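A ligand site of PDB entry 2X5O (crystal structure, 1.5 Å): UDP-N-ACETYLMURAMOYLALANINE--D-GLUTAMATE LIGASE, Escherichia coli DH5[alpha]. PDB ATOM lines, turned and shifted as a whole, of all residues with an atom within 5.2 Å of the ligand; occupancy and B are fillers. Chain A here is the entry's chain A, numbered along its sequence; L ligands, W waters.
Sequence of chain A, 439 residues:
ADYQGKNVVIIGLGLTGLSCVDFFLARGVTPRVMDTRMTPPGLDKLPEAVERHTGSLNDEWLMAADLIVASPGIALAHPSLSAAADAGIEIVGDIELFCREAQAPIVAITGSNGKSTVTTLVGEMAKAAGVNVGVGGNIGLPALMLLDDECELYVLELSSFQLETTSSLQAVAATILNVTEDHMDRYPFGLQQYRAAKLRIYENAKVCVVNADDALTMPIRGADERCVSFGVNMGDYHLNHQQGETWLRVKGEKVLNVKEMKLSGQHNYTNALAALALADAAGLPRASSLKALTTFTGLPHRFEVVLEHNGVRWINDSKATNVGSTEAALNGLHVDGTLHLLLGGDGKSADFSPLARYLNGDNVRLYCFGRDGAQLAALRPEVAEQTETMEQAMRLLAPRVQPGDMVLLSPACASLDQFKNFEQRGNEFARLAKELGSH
S1 of the ligand lies close to NH2 of Arg 37 (3.7 Å).
NZ of Lys 348 lies within salt-bridge range of O4 of the ligand (2.8 Å).
The backbone NH (N) of Ser 415 sits at hydrogen-bond distance from an oxygen (O2) of the ligand, at 2.8 Å.
An oxygen (O7) of the ligand sits at hydrogen-bond distance from the backbone NH (N) of Thr 36 (3.0 Å).
The side-chain hydroxyl (OG) of Ser 415 is in hydrogen-bond range of an oxygen (O2) of the ligand, at 2.6 Å.
The backbone NH (N) of Phe 422 is in hydrogen-bond range of an oxygen (O1) of the ligand, at 2.9 Å.
A nitrogen (N3) of the ligand sits at hydrogen-bond distance from the side-chain hydroxyl of Thr 36.
OD1 of Asn 421 sits close to N of Glu 423 (3.3 Å).
The side-chain hydroxyl (OG) of Ser 71 lies within hydrogen-bond range of the backbone NH (N) of Gly 73.
OD1 of Asp 35 is in salt-bridge range of NE of Arg 37, at 2.9 Å.
The backbone NH (N) of Gly 12 lies within hydrogen-bond range of the backbone carbonyl oxygen (O) of Met 34.
The guanidinium group of Arg 186 lies within hydrogen-bond range of the backbone carbonyl oxygen of Ile 74 (3.2 Å).
N of Ser 71 sits at hydrogen-bond distance from O of Ile 11 (2.9 Å).
The side-chain hydroxyl (OG) of Ser 415 lies close to the backbone carbonyl oxygen (O) of Asn 421, 3.2 Å away.
A ring nitrogen (NE2) of His 183 lies within hydrogen-bond range of the side-chain carboxylate (OD2) of Asp 182 (3.3 Å).
An oxygen (O7) of the ligand lies close to the side-chain carboxylate of Asp 35 (3.4 Å).
CG2 of Ile 11 touches O7 of the ligand, 3.8 Å away.
Gly 12 touches the ligand (CA to S1, 3.8 Å).
Ser 71 touches the ligand.
O of Pro 72 touches C9 of the ligand, at 3.4 Å.
CA of Gly 73 touches C17 of the ligand, 3.7 Å away.
Ile 74 touches the ligand.
Phe 161 touches the ligand (CD2 to C8, 3.5 Å).
His 183 touches the ligand.
Arg 186 touches the ligand (NH1 to C9, 3.7 Å).
CB of Ala 414 touches O4 of the ligand, at 3.4 Å.
CG of Leu 416 touches C2 of the ligand (3.7 Å).
CA of Asn 421 touches O1 of the ligand (3.4 Å).
The nearest printed residue that does not touch the ligand is Thr 321 (4.003 Å).
Water W4 lies within hydrogen-bond range of O3 of the ligand (2.7 Å), OG1 of Thr 321 (2.7 Å), OD2 of Asp 182 (2.8 Å) and NZ of Lys 348 (2.9 Å).
Water W6 lies within hydrogen-bond range of an oxygen (O5) of the ligand (2.9 Å) and the guanidinium group (NH1) of Arg 186 (3.1 Å).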
ATOM      1  N   ILE A  11       9.328  -4.711  20.718  1.00  0.00           N
ATOM      2  CA  ILE A  11       8.386  -3.824  21.424  1.00  0.00           C
ATOM      3  C   ILE A  11       8.295  -2.533  20.644  1.00  0.00           C
ATOM      4  O   ILE A  11       9.309  -1.843  20.429  1.00  0.00           O
ATOM      5  CB  ILE A  11       8.906  -3.425  22.812  1.00  0.00           C
ATOM      6  CG1 ILE A  11       9.203  -4.680  23.636  1.00  0.00           C
ATOM      7  CG2 ILE A  11       7.862  -2.502  23.521  1.00  0.00           C
ATOM      8  CD1 ILE A  11       9.772  -4.332  24.975  1.00  0.00           C
ATOM      9  N   GLY A  12       7.076  -2.252  20.145  1.00  0.00           N
ATOM     10  CA  GLY A  12       6.846  -0.994  19.387  1.00  0.00           C
ATOM     11  C   GLY A  12       6.734  -1.299  17.914  1.00  0.00           C
ATOM     12  O   GLY A  12       7.631  -1.884  17.300  1.00  0.00           O
ATOM     13  N   LEU A  13       5.604  -0.909  17.346  1.00  0.00           N
ATOM     14  CA  LEU A  13       5.380  -1.169  15.921  1.00  0.00           C
ATOM     15  C   LEU A  13       5.765   0.075  15.119  1.00  0.00           C
ATOM     16  O   LEU A  13       6.933   0.485  15.185  1.00  0.00           O
ATOM     17  CB  LEU A  13       3.941  -1.644  15.686  1.00  0.00           C
ATOM     18  CG  LEU A  13       3.827  -2.329  14.323  1.00  0.00           C
ATOM     19  CD1 LEU A  13       4.827  -3.454  14.079  1.00  0.00           C
ATOM     20  CD2 LEU A  13       2.450  -2.844  14.135  1.00  0.00           C
ATOM     21  N   MET A  34       4.977  -6.788  20.480  1.00  0.00           N
ATOM     22  CA  MET A  34       4.052  -6.198  21.427  1.00  0.00           C
ATOM     23  C   MET A  34       4.169  -4.655  21.394  1.00  0.00           C
ATOM     24  O   MET A  34       5.197  -4.072  20.985  1.00  0.00           O
ATOM     25  CB  MET A  34       4.268  -6.763  22.828  1.00  0.00           C
ATOM     26  CG  MET A  34       5.626  -6.368  23.390  1.00  0.00           C
ATOM     27  SD  MET A  34       5.902  -7.062  25.056  1.00  0.00           S
ATOM     28  CE  MET A  34       5.930  -8.824  24.646  1.00  0.00           C
ATOM     29  N   ASP A  35       3.084  -4.002  21.800  1.00  0.00           N
ATOM     30  CA  ASP A  35       3.052  -2.549  21.814  1.00  0.00           C
ATOM     31  C   ASP A  35       2.053  -2.156  22.876  1.00  0.00           C
ATOM     32  O   ASP A  35       0.973  -2.746  22.934  1.00  0.00           O
ATOM     33  CB  ASP A  35       2.655  -2.057  20.407  1.00  0.00           C
ATOM     34  CG  ASP A  35       2.876  -0.544  20.213  1.00  0.00           C
ATOM     35  OD1 ASP A  35       2.317   0.267  20.974  1.00  0.00           O
ATOM     36  OD2 ASP A  35       3.529  -0.183  19.229  1.00  0.00           O
ATOM     37  N   THR A  36       2.381  -1.209  23.732  1.00  0.00           N
ATOM     38  CA  THR A  36       1.461  -0.833  24.790  1.00  0.00           C
ATOM     39  C   THR A  36       0.224  -0.111  24.272  1.00  0.00           C
ATOM     40  O   THR A  36      -0.728   0.019  24.984  1.00  0.00           O
ATOM     41  CB  THR A  36       2.105   0.006  25.936  1.00  0.00           C
ATOM     42  OG1 THR A  36       2.422   1.313  25.435  1.00  0.00           O
ATOM     43  CG2 THR A  36       3.339  -0.717  26.526  1.00  0.00           C
ATOM     44  N   ARG A  37       0.300   0.401  23.044  1.00  0.00           N
ATOM     45  CA  ARG A  37      -0.890   1.063  22.433  1.00  0.00           C
ATOM     46  C   ARG A  37      -1.907   0.011  21.912  1.00  0.00           C
ATOM     47  O   ARG A  37      -1.497  -1.018  21.403  1.00  0.00           O
ATOM     48  CB  ARG A  37      -0.410   1.998  21.316  1.00  0.00           C
ATOM     49  CG  ARG A  37       0.620   3.060  21.832  1.00  0.00           C
ATOM     50  CD  ARG A  37       1.298   3.821  20.683  1.00  0.00           C
ATOM     51  NE  ARG A  37       2.310   3.013  20.017  1.00  0.00           N
ATOM     52  CZ  ARG A  37       3.145   3.443  19.057  1.00  0.00           C
ATOM     53  NH1 ARG A  37       3.144   4.725  18.658  1.00  0.00           N
ATOM     54  NH2 ARG A  37       3.959   2.605  18.483  1.00  0.00           N
ATOM     55  N   LEU A  57       2.330  -4.414  27.777  1.00  0.00           N
ATOM     56  CA  LEU A  57       3.450  -5.364  27.559  1.00  0.00           C
ATOM     57  C   LEU A  57       3.034  -6.705  28.150  1.00  0.00           C
ATOM     58  O   LEU A  57       2.181  -6.781  29.021  1.00  0.00           O
ATOM     59  CB  LEU A  57       4.752  -4.886  28.194  1.00  0.00           C
ATOM     60  CG  LEU A  57       5.309  -3.537  27.694  1.00  0.00           C
ATOM     61  CD1 LEU A  57       6.688  -3.339  28.304  1.00  0.00           C
ATOM     62  CD2 LEU A  57       5.348  -3.549  26.161  1.00  0.00           C
ATOM     63  N   SER A  71      11.814  -0.425  20.883  1.00  0.00           N
ATOM     64  CA  SER A  71      11.683   0.874  20.249  1.00  0.00           C
ATOM     65  C   SER A  71      12.275   1.966  21.136  1.00  0.00           C
ATOM     66  O   SER A  71      12.125   1.916  22.353  1.00  0.00           O
ATOM     67  CB  SER A  71      10.186   1.165  20.068  1.00  0.00           C
ATOM     68  OG  SER A  71       9.994   2.472  19.588  1.00  0.00           O
ATOM     69  N   PRO A  72      12.847   3.001  20.520  1.00  0.00           N
ATOM     70  CA  PRO A  72      13.226   4.145  21.339  1.00  0.00           C
ATOM     71  C   PRO A  72      12.035   4.833  21.990  1.00  0.00           C
ATOM     72  O   PRO A  72      12.222   5.657  22.867  1.00  0.00           O
ATOM     73  CB  PRO A  72      13.933   5.095  20.336  1.00  0.00           C
ATOM     74  CG  PRO A  72      13.358   4.689  18.969  1.00  0.00           C
ATOM     75  CD  PRO A  72      13.159   3.195  19.077  1.00  0.00           C
ATOM     76  N   GLY A  73      10.831   4.506  21.553  1.00  0.00           N
ATOM     77  CA  GLY A  73       9.678   5.185  22.129  1.00  0.00           C
ATOM     78  C   GLY A  73       9.180   4.563  23.432  1.00  0.00           C
ATOM     79  O   GLY A  73       8.371   5.187  24.118  1.00  0.00           O
ATOM     80  N   ILE A  74       9.775   3.473  23.835  1.00  0.00           N
ATOM     81  CA  ILE A  74       9.427   2.828  25.134  1.00  0.00           C
ATOM     82  C   ILE A  74      10.572   2.995  26.134  1.00  0.00           C
ATOM     83  O   ILE A  74      11.738   2.883  25.768  1.00  0.00           O
ATOM     84  CB  ILE A  74       9.039   1.329  24.973  1.00  0.00           C
ATOM     85  CG1 ILE A  74       8.506   0.762  26.307  1.00  0.00           C
ATOM     86  CG2 ILE A  74      10.251   0.489  24.615  1.00  0.00           C
ATOM     87  CD1 ILE A  74       7.039   0.423  26.284  1.00  0.00           C
ATOM     88  N   PHE A 161      17.635   8.238  22.933  1.00  0.00           N
ATOM     89  CA  PHE A 161      16.963   6.972  23.246  1.00  0.00           C
ATOM     90  C   PHE A 161      17.513   5.827  22.426  1.00  0.00           C
ATOM     91  O   PHE A 161      17.719   4.715  22.948  1.00  0.00           O
ATOM     92  CB  PHE A 161      15.429   7.111  23.026  1.00  0.00           C
ATOM     93  CG  PHE A 161      14.850   8.293  23.761  1.00  0.00           C
ATOM     94  CD1 PHE A 161      14.816   8.298  25.157  1.00  0.00           C
ATOM     95  CD2 PHE A 161      14.406   9.372  23.062  1.00  0.00           C
ATOM     96  CE1 PHE A 161      14.225   9.372  25.848  1.00  0.00           C
ATOM     97  CE2 PHE A 161      13.912  10.483  23.747  1.00  0.00           C
ATOM     98  CZ  PHE A 161      13.836  10.472  25.137  1.00  0.00           C
ATOM     99  N   ASP A 182      16.134  18.718  27.539  1.00  0.00           N
ATOM    100  CA  ASP A 182      15.074  18.120  26.737  1.00  0.00           C
ATOM    101  C   ASP A 182      14.724  16.752  27.330  1.00  0.00           C
ATOM    102  O   ASP A 182      15.556  16.122  28.027  1.00  0.00           O
ATOM    103  CB  ASP A 182      15.452  18.076  25.242  1.00  0.00           C
ATOM    104  CG  ASP A 182      14.226  17.895  24.299  1.00  0.00           C
ATOM    105  OD1 ASP A 182      13.108  17.786  24.778  1.00  0.00           O
ATOM    106  OD2 ASP A 182      14.514  17.720  23.069  1.00  0.00           O
ATOM    107  N   HIS A 183      13.531  16.266  27.050  1.00  0.00           N
ATOM    108  CA  HIS A 183      13.180  14.870  27.407  1.00  0.00           C
ATOM    109  C   HIS A 183      13.294  14.613  28.900  1.00  0.00           C
ATOM    110  O   HIS A 183      13.465  13.460  29.287  1.00  0.00           O
ATOM    111  CB  HIS A 183      14.023  13.857  26.608  1.00  0.00           C
ATOM    112  CG  HIS A 183      13.866  14.021  25.136  1.00  0.00           C
ATOM    113  ND1 HIS A 183      12.655  13.826  24.501  1.00  0.00           N
ATOM    114  CD2 HIS A 183      14.765  14.328  24.182  1.00  0.00           C
ATOM    115  CE1 HIS A 183      12.825  14.048  23.198  1.00  0.00           C
ATOM    116  NE2 HIS A 183      14.077  14.408  22.989  1.00  0.00           N
ATOM    117  N   ARG A 186      11.594  11.663  30.474  1.00  0.00           N
ATOM    118  CA  ARG A 186      12.178  10.338  30.230  1.00  0.00           C
ATOM    119  C   ARG A 186      13.551  10.191  30.903  1.00  0.00           C
ATOM    120  O   ARG A 186      14.141   9.135  30.841  1.00  0.00           O
ATOM    121  CB  ARG A 186      12.235  10.037  28.733  1.00  0.00           C
ATOM    122  CG  ARG A 186      10.790   9.786  28.266  1.00  0.00           C
ATOM    123  CD  ARG A 186      10.790   9.164  26.947  1.00  0.00           C
ATOM    124  NE  ARG A 186      11.405   7.828  26.940  1.00  0.00           N
ATOM    125  CZ  ARG A 186      11.598   7.148  25.802  1.00  0.00           C
ATOM    126  NH1 ARG A 186      11.210   7.689  24.675  1.00  0.00           N
ATOM    127  NH2 ARG A 186      12.292   6.039  25.774  1.00  0.00           N
ATOM    128  N   THR A 321      10.967  21.765  19.129  1.00  0.00           N
ATOM    129  CA  THR A 321      10.259  20.964  20.119  1.00  0.00           C
ATOM    130  C   THR A 321      10.893  21.076  21.508  1.00  0.00           C
ATOM    131  O   THR A 321      10.516  20.353  22.417  1.00  0.00           O
ATOM    132  CB  THR A 321      10.233  19.504  19.660  1.00  0.00           C
ATOM    133  OG1 THR A 321      11.592  19.110  19.413  1.00  0.00           O
ATOM    134  CG2 THR A 321       9.405  19.372  18.336  1.00  0.00           C
ATOM    135  N   LYS A 348       7.339  18.543  28.215  1.00  0.00           N
ATOM    136  CA  LYS A 348       8.251  17.464  28.707  1.00  0.00           C
ATOM    137  C   LYS A 348       8.966  17.909  29.965  1.00  0.00           C
ATOM    138  O   LYS A 348      10.112  17.493  30.226  1.00  0.00           O
ATOM    139  CB  LYS A 348       9.256  17.072  27.621  1.00  0.00           C
ATOM    140  CG  LYS A 348       8.599  16.488  26.384  1.00  0.00           C
ATOM    141  CD  LYS A 348       9.582  16.380  25.201  1.00  0.00           C
ATOM    142  CE  LYS A 348       9.665  17.712  24.505  1.00  0.00           C
ATOM    143  NZ  LYS A 348      10.624  17.623  23.393  1.00  0.00           N
ATOM    144  N   CYS A 413       8.051  22.886  22.417  1.00  0.00           N
ATOM    145  CA  CYS A 413       7.320  21.764  23.039  1.00  0.00           C
ATOM    146  C   CYS A 413       7.095  20.675  22.019  1.00  0.00           C
ATOM    147  O   CYS A 413       6.964  20.952  20.820  1.00  0.00           O
ATOM    148  CB  CYS A 413       5.926  22.197  23.527  1.00  0.00           C
ATOM    149  SG  CYS A 413       5.932  23.376  24.835  1.00  0.00           S
ATOM    150  N   ALA A 414       6.985  19.425  22.486  1.00  0.00           N
ATOM    151  CA  ALA A 414       6.454  18.380  21.598  1.00  0.00           C
ATOM    152  C   ALA A 414       5.014  18.676  21.195  1.00  0.00           C
ATOM    153  O   ALA A 414       4.284  19.324  21.920  1.00  0.00           O
ATOM    154  CB  ALA A 414       6.536  17.012  22.281  1.00  0.00           C
ATOM    155  N   SER A 415       4.644  18.152  20.042  1.00  0.00           N
ATOM    156  CA  SER A 415       3.306  18.320  19.482  1.00  0.00           C
ATOM    157  C   SER A 415       2.353  17.181  19.835  1.00  0.00           C
ATOM    158  O   SER A 415       1.151  17.265  19.556  1.00  0.00           O
ATOM    159  CB  SER A 415       3.368  18.433  17.954  1.00  0.00           C
ATOM    160  OG  SER A 415       3.694  17.177  17.418  1.00  0.00           O
ATOM    161  N   LEU A 416       2.857  16.215  20.582  1.00  0.00           N
ATOM    162  CA  LEU A 416       2.234  14.890  20.632  1.00  0.00           C
ATOM    163  C   LEU A 416       0.944  14.836  21.458  1.00  0.00           C
ATOM    164  O   LEU A 416       0.160  13.884  21.316  1.00  0.00           O
ATOM    165  CB  LEU A 416       3.228  13.829  21.097  1.00  0.00           C
ATOM    166  CG  LEU A 416       4.484  13.645  20.209  1.00  0.00           C
ATOM    167  CD1 LEU A 416       5.496  12.583  20.720  1.00  0.00           C
ATOM    168  CD2 LEU A 416       4.151  13.477  18.715  1.00  0.00           C
ATOM    169  N   LYS A 420      -0.081  14.210  15.452  1.00  0.00           N
ATOM    170  CA  LYS A 420       0.731  13.021  15.222  1.00  0.00           C
ATOM    171  C   LYS A 420       2.235  13.288  15.423  1.00  0.00           C
ATOM    172  O   LYS A 420       2.969  12.421  15.952  1.00  0.00           O
ATOM    173  CB  LYS A 420       0.463  12.438  13.843  1.00  0.00           C
ATOM    174  CG  LYS A 420       1.221  11.152  13.582  1.00  0.00           C
ATOM    175  CD  LYS A 420       0.734  10.417  12.320  1.00  0.00           C
ATOM    176  CE  LYS A 420       0.996  11.262  11.066  1.00  0.00           C
ATOM    177  NZ  LYS A 420       0.666  10.517   9.802  1.00  0.00           N
ATOM    178  N   ASN A 421       2.686  14.470  15.011  1.00  0.00           N
ATOM    179  CA  ASN A 421       4.118  14.795  15.034  1.00  0.00           C
ATOM    180  C   ASN A 421       4.257  16.233  14.613  1.00  0.00           C
ATOM    181  O   ASN A 421       3.254  16.867  14.224  1.00  0.00           O
ATOM    182  CB  ASN A 421       4.880  13.879  14.047  1.00  0.00           C
ATOM    183  CG  ASN A 421       4.211  13.788  12.689  1.00  0.00           C
ATOM    184  OD1 ASN A 421       3.801  14.782  12.112  1.00  0.00           O
ATOM    185  ND2 ASN A 421       4.227  12.599  12.114  1.00  0.00           N
ATOM    186  N   PHE A 422       5.471  16.775  14.719  1.00  0.00           N
ATOM    187  CA  PHE A 422       5.640  18.201  14.535  1.00  0.00           C
ATOM    188  C   PHE A 422       5.431  18.552  13.074  1.00  0.00           C
ATOM    189  O   PHE A 422       5.110  19.699  12.774  1.00  0.00           O
ATOM    190  CB  PHE A 422       7.029  18.693  14.990  1.00  0.00           C
ATOM    191  CG  PHE A 422       8.158  18.198  14.092  1.00  0.00           C
ATOM    192  CD1 PHE A 422       8.541  18.919  12.958  1.00  0.00           C
ATOM    193  CD2 PHE A 422       8.829  16.987  14.382  1.00  0.00           C
ATOM    194  CE1 PHE A 422       9.546  18.426  12.112  1.00  0.00           C
ATOM    195  CE2 PHE A 422       9.813  16.451  13.517  1.00  0.00           C
ATOM    196  CZ  PHE A 422      10.202  17.194  12.381  1.00  0.00           C
ATOM    197  N   GLU A 423       5.591  17.594  12.179  1.00  0.00           N
ATOM    198  CA  GLU A 423       5.310  17.866  10.750  1.00  0.00           C
ATOM    199  C   GLU A 423       3.841  18.177  10.558  1.00  0.00           C
ATOM    200  O   GLU A 423       3.494  19.119   9.831  1.00  0.00           O
ATOM    201  CB  GLU A 423       5.656  16.642   9.889  1.00  0.00           C
ATOM    202  CG  GLU A 423       7.148  16.477   9.688  1.00  0.00           C
ATOM    203  CD  GLU A 423       7.783  15.575  10.726  1.00  0.00           C
ATOM    204  OE1 GLU A 423       7.158  15.287  11.768  1.00  0.00           O
ATOM    205  OE2 GLU A 423       8.946  15.162  10.496  1.00  0.00           O
ATOM    206  N   ARG A 425       1.792  19.387  12.781  1.00  0.00           N
ATOM    207  CA  ARG A 425       1.622  20.704  13.376  1.00  0.00           C
ATOM    208  C   ARG A 425       2.084  21.812  12.452  1.00  0.00           C
ATOM    209  O   ARG A 425       1.338  22.769  12.225  1.00  0.00           O
ATOM    210  CB  ARG A 425       2.293  20.757  14.750  1.00  0.00           C
ATOM    211  CG  ARG A 425       2.342  22.154  15.384  1.00  0.00           C
ATOM    212  CD  ARG A 425       2.967  22.066  16.793  1.00  0.00           C
ATOM    213  NE  ARG A 425       4.411  21.789  16.745  1.00  0.00           N
ATOM    214  CZ  ARG A 425       5.150  21.509  17.801  1.00  0.00           C
ATOM    215  NH1 ARG A 425       4.595  21.465  19.010  1.00  0.00           N
ATOM    216  NH2 ARG A 425       6.466  21.367  17.636  1.00  0.00           N
HETATM  217  O1  LIG L   1       7.008  15.346  16.746  1.00  0.00           O
HETATM  218  C1  LIG L   1       6.923  15.966  17.853  1.00  0.00           C
HETATM  219  O2  LIG L   1       6.209  16.980  18.041  1.00  0.00           O
HETATM  220  C2  LIG L   1       7.535  15.497  19.100  1.00  0.00           C
HETATM  221  C3  LIG L   1       8.550  14.457  18.825  1.00  0.00           C
HETATM  222  C4  LIG L   1      10.095  14.975  20.782  1.00  0.00           C
HETATM  223  O3  LIG L   1      11.300  15.042  20.490  1.00  0.00           O
HETATM  224  O4  LIG L   1       9.643  15.642  21.744  1.00  0.00           O
HETATM  225  N1  LIG L   1       9.742  12.731  19.930  1.00  0.00           N
HETATM  226  C5  LIG L   1      10.039  11.884  21.052  1.00  0.00           C
HETATM  227  O5  LIG L   1      10.054  12.295  22.216  1.00  0.00           O
HETATM  228  C6  LIG L   1      10.435  10.526  20.621  1.00  0.00           C
HETATM  229  C7  LIG L   1       9.852   9.990  19.453  1.00  0.00           C
HETATM  230  C8  LIG L   1      11.287   9.765  21.416  1.00  0.00           C
HETATM  231  C9  LIG L   1      11.572   8.464  21.058  1.00  0.00           C
HETATM  232  C10 LIG L   1      11.041   7.926  19.926  1.00  0.00           C
HETATM  233  C11 LIG L   1      10.175   8.657  19.115  1.00  0.00           C
HETATM  234  C12 LIG L   1       9.722   8.024  17.806  1.00  0.00           C
HETATM  235  N2  LIG L   1       9.386   6.692  17.909  1.00  0.00           N
HETATM  236  C13 LIG L   1       8.362   6.229  18.682  1.00  0.00           C
HETATM  237  C14 LIG L   1       7.575   7.094  19.460  1.00  0.00           C
HETATM  238  C15 LIG L   1       6.601   6.613  20.333  1.00  0.00           C
HETATM  239  C16 LIG L   1       8.118   4.853  18.746  1.00  0.00           C
HETATM  240  C17 LIG L   1       7.131   4.357  19.611  1.00  0.00           C
HETATM  241  C18 LIG L   1       6.403   5.219  20.419  1.00  0.00           C
HETATM  242  C19 LIG L   1       5.373   4.748  21.421  1.00  0.00           C
HETATM  243  C20 LIG L   1       5.147   3.508  21.958  1.00  0.00           C
HETATM  244  S1  LIG L   1       5.960   2.008  21.597  1.00  0.00           S
HETATM  245  C21 LIG L   1       4.959   1.161  22.737  1.00  0.00           C
HETATM  246  N3  LIG L   1       4.091   1.926  23.502  1.00  0.00           N
HETATM  247  C22 LIG L   1       9.078  13.982  20.196  1.00  0.00           C
HETATM  248  C23 LIG L   1       4.219   3.252  23.054  1.00  0.00           C
HETATM  249  O6  LIG L   1       3.498   4.146  23.467  1.00  0.00           O
HETATM  250  O7  LIG L   1       5.065  -0.031  22.974  1.00  0.00           O
HETATM  251  O   HOH W   1       7.856  13.705  23.758  1.00  0.00           O
HETATM  252  O   HOH W   2       8.122  13.196  15.834  1.00  0.00           O
HETATM  253  O   HOH W   3       6.793   9.769  21.806  1.00  0.00           O
HETATM  254  O   HOH W   4      12.508  17.298  21.190  1.00  0.00           O
HETATM  255  O   HOH W   5      11.718   9.961  15.852  1.00  0.00           O
HETATM  256  O   HOH W   6       9.524  10.287  24.184  1.00  0.00           O
HETATM  257  O   HOH W   7      11.117   5.023  16.193  1.00  0.00           O
HETATM  258  O   HOH W   8      10.485  12.368  17.088  1.00  0.00           O
